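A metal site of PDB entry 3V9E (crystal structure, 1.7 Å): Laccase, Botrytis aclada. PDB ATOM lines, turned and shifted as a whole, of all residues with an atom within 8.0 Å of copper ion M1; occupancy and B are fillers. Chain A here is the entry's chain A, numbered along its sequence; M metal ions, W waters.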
ATOM      1  N   HIS A 124      -4.012 -22.751 -32.270  1.00  0.00           N
ATOM      2  CA  HIS A 124      -2.928 -22.471 -31.391  1.00  0.00           C
ATOM      3  C   HIS A 124      -1.589 -22.981 -31.966  1.00  0.00           C
ATOM      4  O   HIS A 124      -1.574 -23.977 -32.626  1.00  0.00           O
ATOM      5  CB  HIS A 124      -3.198 -23.167 -30.066  1.00  0.00           C
ATOM      6  CG  HIS A 124      -2.052 -23.186 -29.133  1.00  0.00           C
ATOM      7  ND1 HIS A 124      -1.545 -22.041 -28.574  1.00  0.00           N
ATOM      8  CD2 HIS A 124      -1.337 -24.210 -28.590  1.00  0.00           C
ATOM      9  CE1 HIS A 124      -0.545 -22.343 -27.759  1.00  0.00           C
ATOM     10  NE2 HIS A 124      -0.411 -23.661 -27.743  1.00  0.00           N
ATOM     11  N   TRP A 125      -0.540 -22.219 -31.667  1.00  0.00           N
ATOM     12  CA  TRP A 125       0.848 -22.432 -32.183  1.00  0.00           C
ATOM     13  C   TRP A 125       1.565 -22.956 -30.939  1.00  0.00           C
ATOM     14  O   TRP A 125       1.890 -22.189 -30.046  1.00  0.00           O
ATOM     15  CB  TRP A 125       1.402 -21.129 -32.795  1.00  0.00           C
ATOM     16  CG  TRP A 125       0.257 -20.458 -33.506  1.00  0.00           C
ATOM     17  CD1 TRP A 125      -0.573 -19.509 -32.993  1.00  0.00           C
ATOM     18  CD2 TRP A 125      -0.197 -20.731 -34.817  1.00  0.00           C
ATOM     19  NE1 TRP A 125      -1.536 -19.170 -33.901  1.00  0.00           N
ATOM     20  CE2 TRP A 125      -1.392 -19.969 -35.002  1.00  0.00           C
ATOM     21  CE3 TRP A 125       0.222 -21.603 -35.832  1.00  0.00           C
ATOM     22  CZ2 TRP A 125      -2.114 -20.016 -36.142  1.00  0.00           C
ATOM     23  CZ3 TRP A 125      -0.558 -21.689 -36.962  1.00  0.00           C
ATOM     24  CH2 TRP A 125      -1.728 -20.896 -37.131  1.00  0.00           C
ATOM     25  N   HIS A 126       1.706 -24.296 -30.888  1.00  0.00           N
ATOM     26  CA  HIS A 126       1.994 -24.947 -29.650  1.00  0.00           C
ATOM     27  C   HIS A 126       3.374 -24.553 -29.183  1.00  0.00           C
ATOM     28  O   HIS A 126       4.388 -24.760 -29.860  1.00  0.00           O
ATOM     29  CB  HIS A 126       1.833 -26.460 -29.749  1.00  0.00           C
ATOM     30  CG  HIS A 126       2.003 -27.104 -28.437  1.00  0.00           C
ATOM     31  ND1 HIS A 126       0.982 -27.715 -27.767  1.00  0.00           N
ATOM     32  CD2 HIS A 126       3.094 -27.216 -27.657  1.00  0.00           C
ATOM     33  CE1 HIS A 126       1.435 -28.213 -26.645  1.00  0.00           C
ATOM     34  NE2 HIS A 126       2.702 -27.885 -26.530  1.00  0.00           N
ATOM     35  N   GLY A 127       3.444 -24.080 -27.940  1.00  0.00           N
ATOM     36  CA  GLY A 127       4.713 -23.749 -27.297  1.00  0.00           C
ATOM     37  C   GLY A 127       5.223 -22.413 -27.669  1.00  0.00           C
ATOM     38  O   GLY A 127       6.323 -22.031 -27.240  1.00  0.00           O
ATOM     39  N   ASP A 137      -2.497 -16.298 -29.628  1.00  0.00           N
ATOM     40  CA  ASP A 137      -2.230 -17.615 -29.074  1.00  0.00           C
ATOM     41  C   ASP A 137      -3.217 -18.713 -29.467  1.00  0.00           C
ATOM     42  O   ASP A 137      -2.942 -19.929 -29.339  1.00  0.00           O
ATOM     43  CB  ASP A 137      -2.184 -17.497 -27.513  1.00  0.00           C
ATOM     44  CG  ASP A 137      -1.565 -18.664 -26.857  1.00  0.00           C
ATOM     45  OD1 ASP A 137      -0.533 -19.151 -27.368  1.00  0.00           O
ATOM     46  OD2 ASP A 137      -2.073 -19.083 -25.795  1.00  0.00           O
ATOM     47  N   GLY A 138      -4.418 -18.293 -29.844  1.00  0.00           N
ATOM     48  CA  GLY A 138      -5.395 -19.193 -30.425  1.00  0.00           C
ATOM     49  C   GLY A 138      -6.238 -19.989 -29.479  1.00  0.00           C
ATOM     50  O   GLY A 138      -6.762 -21.042 -29.861  1.00  0.00           O
ATOM     51  N   VAL A 139      -6.456 -19.500 -28.254  1.00  0.00           N
ATOM     52  CA  VAL A 139      -7.245 -20.271 -27.303  1.00  0.00           C
ATOM     53  C   VAL A 139      -8.632 -19.609 -27.242  1.00  0.00           C
ATOM     54  O   VAL A 139      -8.695 -18.513 -26.680  1.00  0.00           O
ATOM     55  CB  VAL A 139      -6.689 -20.246 -25.953  1.00  0.00           C
ATOM     56  CG1 VAL A 139      -7.538 -21.026 -25.020  1.00  0.00           C
ATOM     57  CG2 VAL A 139      -5.287 -20.922 -25.943  1.00  0.00           C
ATOM     58  N   TRP A 166       4.186 -27.878 -33.308  1.00  0.00           N
ATOM     59  CA  TRP A 166       3.052 -28.171 -34.115  1.00  0.00           C
ATOM     60  C   TRP A 166       2.006 -27.082 -33.871  1.00  0.00           C
ATOM     61  O   TRP A 166       2.129 -26.359 -32.897  1.00  0.00           O
ATOM     62  CB  TRP A 166       2.492 -29.537 -33.792  1.00  0.00           C
ATOM     63  CG  TRP A 166       2.047 -29.836 -32.344  1.00  0.00           C
ATOM     64  CD1 TRP A 166       2.728 -29.596 -31.185  1.00  0.00           C
ATOM     65  CD2 TRP A 166       0.801 -30.416 -31.929  1.00  0.00           C
ATOM     66  NE1 TRP A 166       2.022 -30.011 -30.082  1.00  0.00           N
ATOM     67  CE2 TRP A 166       0.866 -30.587 -30.523  1.00  0.00           C
ATOM     68  CE3 TRP A 166      -0.301 -30.891 -32.604  1.00  0.00           C
ATOM     69  CZ2 TRP A 166      -0.212 -31.063 -29.779  1.00  0.00           C
ATOM     70  CZ3 TRP A 166      -1.316 -31.410 -31.910  1.00  0.00           C
ATOM     71  CH2 TRP A 166      -1.307 -31.500 -30.514  1.00  0.00           C
ATOM     72  N   HIS A 168      -2.320 -26.450 -33.959  1.00  0.00           N
ATOM     73  CA  HIS A 168      -3.504 -27.255 -33.901  1.00  0.00           C
ATOM     74  C   HIS A 168      -4.656 -26.465 -33.400  1.00  0.00           C
ATOM     75  O   HIS A 168      -4.514 -25.465 -32.706  1.00  0.00           O
ATOM     76  CB  HIS A 168      -3.364 -28.476 -33.018  1.00  0.00           C
ATOM     77  CG  HIS A 168      -2.966 -28.187 -31.600  1.00  0.00           C
ATOM     78  ND1 HIS A 168      -3.889 -27.937 -30.594  1.00  0.00           N
ATOM     79  CD2 HIS A 168      -1.757 -28.246 -30.989  1.00  0.00           C
ATOM     80  CE1 HIS A 168      -3.254 -27.786 -29.439  1.00  0.00           C
ATOM     81  NE2 HIS A 168      -1.951 -27.982 -29.643  1.00  0.00           N
ATOM     82  N   SER A 169      -5.801 -26.965 -33.725  1.00  0.00           N
ATOM     83  CA  SER A 169      -6.974 -26.353 -33.178  1.00  0.00           C
ATOM     84  C   SER A 169      -6.992 -26.490 -31.669  1.00  0.00           C
ATOM     85  O   SER A 169      -6.648 -27.519 -31.138  1.00  0.00           O
ATOM     86  CB  SER A 169      -8.260 -26.921 -33.731  1.00  0.00           C
ATOM     87  OG  SER A 169      -9.361 -26.319 -33.008  1.00  0.00           O
ATOM     88  N   HIS A 170      -7.413 -25.407 -30.991  1.00  0.00           N
ATOM     89  CA  HIS A 170      -7.586 -25.483 -29.541  1.00  0.00           C
ATOM     90  C   HIS A 170      -9.060 -25.258 -29.229  1.00  0.00           C
ATOM     91  O   HIS A 170      -9.406 -24.956 -28.092  1.00  0.00           O
ATOM     92  CB  HIS A 170      -6.744 -24.395 -28.884  1.00  0.00           C
ATOM     93  CG  HIS A 170      -6.113 -24.816 -27.612  1.00  0.00           C
ATOM     94  ND1 HIS A 170      -6.848 -25.257 -26.574  1.00  0.00           N
ATOM     95  CD2 HIS A 170      -4.820 -24.903 -27.204  1.00  0.00           C
ATOM     96  CE1 HIS A 170      -6.078 -25.550 -25.548  1.00  0.00           C
ATOM     97  NE2 HIS A 170      -4.834 -25.375 -25.917  1.00  0.00           N
ATOM     98  N   ILE A 465       0.748 -31.847 -18.895  1.00  0.00           N
ATOM     99  CA  ILE A 465       0.297 -30.505 -18.574  1.00  0.00           C
ATOM    100  C   ILE A 465       1.033 -29.521 -19.492  1.00  0.00           C
ATOM    101  O   ILE A 465       2.294 -29.494 -19.521  1.00  0.00           O
ATOM    102  CB  ILE A 465       0.652 -30.143 -17.118  1.00  0.00           C
ATOM    103  CG1 ILE A 465       0.009 -31.157 -16.140  1.00  0.00           C
ATOM    104  CG2 ILE A 465       0.321 -28.683 -16.819  1.00  0.00           C
ATOM    105  CD1 ILE A 465      -1.523 -31.193 -16.173  1.00  0.00           C
ATOM    106  N   HIS A 466       0.217 -28.732 -20.197  1.00  0.00           N
ATOM    107  CA  HIS A 466       0.720 -27.730 -21.132  1.00  0.00           C
ATOM    108  C   HIS A 466       0.503 -26.346 -20.546  1.00  0.00           C
ATOM    109  O   HIS A 466      -0.587 -26.041 -20.184  1.00  0.00           O
ATOM    110  CB  HIS A 466      -0.024 -27.856 -22.459  1.00  0.00           C
ATOM    111  CG  HIS A 466       0.379 -26.838 -23.467  1.00  0.00           C
ATOM    112  ND1 HIS A 466      -0.488 -26.295 -24.411  1.00  0.00           N
ATOM    113  CD2 HIS A 466       1.578 -26.232 -23.647  1.00  0.00           C
ATOM    114  CE1 HIS A 466       0.172 -25.407 -25.121  1.00  0.00           C
ATOM    115  NE2 HIS A 466       1.418 -25.368 -24.698  1.00  0.00           N
ATOM    116  N   LEU A 467       1.531 -25.531 -20.497  1.00  0.00           N
ATOM    117  CA  LEU A 467       1.425 -24.126 -20.120  1.00  0.00           C
ATOM    118  C   LEU A 467       1.669 -23.221 -21.358  1.00  0.00           C
ATOM    119  O   LEU A 467       2.661 -23.350 -22.014  1.00  0.00           O
ATOM    120  CB  LEU A 467       2.500 -23.746 -19.109  1.00  0.00           C
ATOM    121  CG  LEU A 467       2.583 -22.245 -18.734  1.00  0.00           C
ATOM    122  CD1 LEU A 467       1.357 -21.717 -18.083  1.00  0.00           C
ATOM    123  CD2 LEU A 467       3.701 -21.955 -17.696  1.00  0.00           C
ATOM    124  N   HIS A 468       0.753 -22.311 -21.589  1.00  0.00           N
ATOM    125  CA  HIS A 468       0.833 -21.370 -22.699  1.00  0.00           C
ATOM    126  C   HIS A 468       1.716 -20.160 -22.274  1.00  0.00           C
ATOM    127  O   HIS A 468       1.820 -19.804 -21.082  1.00  0.00           O
ATOM    128  CB  HIS A 468      -0.581 -20.938 -23.082  1.00  0.00           C
ATOM    129  CG  HIS A 468      -1.370 -21.994 -23.755  1.00  0.00           C
ATOM    130  ND1 HIS A 468      -2.008 -21.776 -24.961  1.00  0.00           N
ATOM    131  CD2 HIS A 468      -1.660 -23.256 -23.410  1.00  0.00           C
ATOM    132  CE1 HIS A 468      -2.585 -22.902 -25.360  1.00  0.00           C
ATOM    133  NE2 HIS A 468      -2.395 -23.818 -24.426  1.00  0.00           N
ATOM    134  N   ASP A 500       7.607 -27.038 -22.355  1.00  0.00           N
ATOM    135  CA  ASP A 500       6.223 -26.518 -22.253  1.00  0.00           C
ATOM    136  C   ASP A 500       5.133 -27.495 -22.029  1.00  0.00           C
ATOM    137  O   ASP A 500       3.957 -27.106 -21.758  1.00  0.00           O
ATOM    138  CB  ASP A 500       5.911 -25.581 -23.457  1.00  0.00           C
ATOM    139  CG  ASP A 500       5.942 -26.297 -24.775  1.00  0.00           C
ATOM    140  OD1 ASP A 500       5.106 -27.207 -24.982  1.00  0.00           O
ATOM    141  OD2 ASP A 500       6.806 -25.947 -25.626  1.00  0.00           O
ATOM    142  N   VAL A 501       5.468 -28.774 -22.086  1.00  0.00           N
ATOM    143  CA  VAL A 501       4.486 -29.836 -21.688  1.00  0.00           C
ATOM    144  C   VAL A 501       5.246 -30.781 -20.769  1.00  0.00           C
ATOM    145  O   VAL A 501       6.356 -31.271 -21.083  1.00  0.00           O
ATOM    146  CB  VAL A 501       3.903 -30.617 -22.866  1.00  0.00           C
ATOM    147  CG1 VAL A 501       3.039 -31.791 -22.380  1.00  0.00           C
ATOM    148  CG2 VAL A 501       3.091 -29.703 -23.756  1.00  0.00           C
ATOM    149  N   LEU A 523      -3.449 -20.015 -20.623  1.00  0.00           N
ATOM    150  CA  LEU A 523      -4.047 -21.265 -20.278  1.00  0.00           C
ATOM    151  C   LEU A 523      -3.004 -22.308 -19.816  1.00  0.00           C
ATOM    152  O   LEU A 523      -1.937 -22.376 -20.328  1.00  0.00           O
ATOM    153  CB  LEU A 523      -4.806 -21.787 -21.514  1.00  0.00           C
ATOM    154  CG  LEU A 523      -5.699 -22.994 -21.244  1.00  0.00           C
ATOM    155  CD1 LEU A 523      -6.922 -22.595 -20.423  1.00  0.00           C
ATOM    156  CD2 LEU A 523      -6.142 -23.657 -22.547  1.00  0.00           C
ATOM    157  N   LEU A 524      -3.373 -23.104 -18.801  1.00  0.00           N
ATOM    158  CA  LEU A 524      -2.631 -24.283 -18.419  1.00  0.00           C
ATOM    159  C   LEU A 524      -3.645 -25.420 -18.299  1.00  0.00           C
ATOM    160  O   LEU A 524      -4.721 -25.283 -17.732  1.00  0.00           O
ATOM    161  CB  LEU A 524      -1.871 -24.087 -17.098  1.00  0.00           C
ATOM    162  CG  LEU A 524      -1.178 -25.344 -16.528  1.00  0.00           C
ATOM    163  CD1 LEU A 524       0.065 -24.958 -15.740  1.00  0.00           C
ATOM    164  CD2 LEU A 524      -2.197 -26.119 -15.665  1.00  0.00           C
ATOM    165  N   HIS A 525      -3.327 -26.547 -18.889  1.00  0.00           N
ATOM    166  CA  HIS A 525      -4.255 -27.616 -18.985  1.00  0.00           C
ATOM    167  C   HIS A 525      -3.635 -28.920 -19.281  1.00  0.00           C
ATOM    168  O   HIS A 525      -2.539 -29.010 -19.832  1.00  0.00           O
ATOM    169  CB  HIS A 525      -5.284 -27.300 -20.082  1.00  0.00           C
ATOM    170  CG  HIS A 525      -4.674 -27.239 -21.457  1.00  0.00           C
ATOM    171  ND1 HIS A 525      -4.799 -28.301 -22.331  1.00  0.00           N
ATOM    172  CD2 HIS A 525      -3.950 -26.292 -22.093  1.00  0.00           C
ATOM    173  CE1 HIS A 525      -4.187 -27.975 -23.475  1.00  0.00           C
ATOM    174  NE2 HIS A 525      -3.654 -26.767 -23.344  1.00  0.00           N
ATOM    175  N   CYS A 526      -4.397 -29.968 -18.972  1.00  0.00           N
ATOM    176  CA  CYS A 526      -4.081 -31.297 -19.374  1.00  0.00           C
ATOM    177  C   CYS A 526      -4.314 -31.390 -20.874  1.00  0.00           C
ATOM    178  O   CYS A 526      -5.372 -30.934 -21.337  1.00  0.00           O
ATOM    179  CB  CYS A 526      -4.942 -32.338 -18.672  1.00  0.00           C
ATOM    180  SG  CYS A 526      -4.456 -34.005 -19.163  1.00  0.00           S
ATOM    181  N   HIS A 527      -3.409 -32.059 -21.573  1.00  0.00           N
ATOM    182  CA  HIS A 527      -3.481 -32.129 -23.061  1.00  0.00           C
ATOM    183  C   HIS A 527      -4.154 -33.404 -23.498  1.00  0.00           C
ATOM    184  O   HIS A 527      -4.304 -33.605 -24.676  1.00  0.00           O
ATOM    185  CB  HIS A 527      -2.055 -32.017 -23.682  1.00  0.00           C
ATOM    186  CG  HIS A 527      -1.989 -31.271 -24.981  1.00  0.00           C
ATOM    187  ND1 HIS A 527      -2.698 -31.649 -26.101  1.00  0.00           N
ATOM    188  CD2 HIS A 527      -1.243 -30.185 -25.354  1.00  0.00           C
ATOM    189  CE1 HIS A 527      -2.402 -30.848 -27.113  1.00  0.00           C
ATOM    190  NE2 HIS A 527      -1.525 -29.932 -26.683  1.00  0.00           N
ATOM    191  N   ALA A 532      -9.127 -32.115 -21.036  1.00  0.00           N
ATOM    192  CA  ALA A 532      -9.277 -30.701 -21.304  1.00  0.00           C
ATOM    193  C   ALA A 532     -10.731 -30.296 -21.495  1.00  0.00           C
ATOM    194  O   ALA A 532     -11.232 -29.306 -20.988  1.00  0.00           O
ATOM    195  CB  ALA A 532      -8.441 -30.326 -22.546  1.00  0.00           C
ATOM    196  N   ILE A 580     -12.125 -25.469 -24.349  1.00  0.00           N
ATOM    197  CA  ILE A 580     -10.717 -25.420 -24.828  1.00  0.00           C
ATOM    198  C   ILE A 580     -10.321 -26.723 -25.365  1.00  0.00           C
ATOM    199  O   ILE A 580     -11.251 -27.550 -25.548  1.00  0.00           O
ATOM    200  CB  ILE A 580      -9.766 -24.910 -23.747  1.00  0.00           C
ATOM    201  CG1 ILE A 580     -10.045 -25.561 -22.372  1.00  0.00           C
ATOM    202  CG2 ILE A 580      -9.909 -23.397 -23.577  1.00  0.00           C
ATOM    203  CD1 ILE A 580      -9.346 -26.823 -22.081  1.00  0.00           C
ATOM    204  OXT ILE A 580      -9.075 -26.892 -25.597  1.00  0.00           O
HETATM  205 CU    CU M   1      -2.995 -25.640 -24.814  1.00  0.00          CU
HETATM  206 CU    CU M   2      -0.744 -28.244 -28.073  1.00  0.00          CU
HETATM  207  O   HOH W   1      -2.693 -27.033 -26.256  1.00  0.00           O
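The backbone NH (N) of His 468 sits at hydrogen-bond distance from the backbone carbonyl oxygen (O) of Leu 523, at 3.0 Å. OD2 of Asp 137 is in hydrogen-bond range of ND1 of His 468. NE2 of His 468 sits close to ND1 of His 466 (3.1 Å). O of His 525 sits at hydrogen-bond distance from N of His 466, at 2.8 Å. A ring nitrogen (NE2) of His 466 lies within hydrogen-bond range of a ring nitrogen (NE2) of His 126 (3.4 Å). OXT of Ile 580 sits at hydrogen-bond distance from ND1 of His 170 (2.9 Å).
The nearest printed residue that does not touch copper ion M1 is Leu 523 (4.4 Å).
Copper ion M1 is bound by a ring nitrogen (NE2) of His 468, a ring nitrogen (NE2) of His 525, water W1 and a ring nitrogen (NE2) of His 170. Slightly farther from copper ion M1 lies a ring nitrogen (ND1) of His 466 (2.6 Å).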
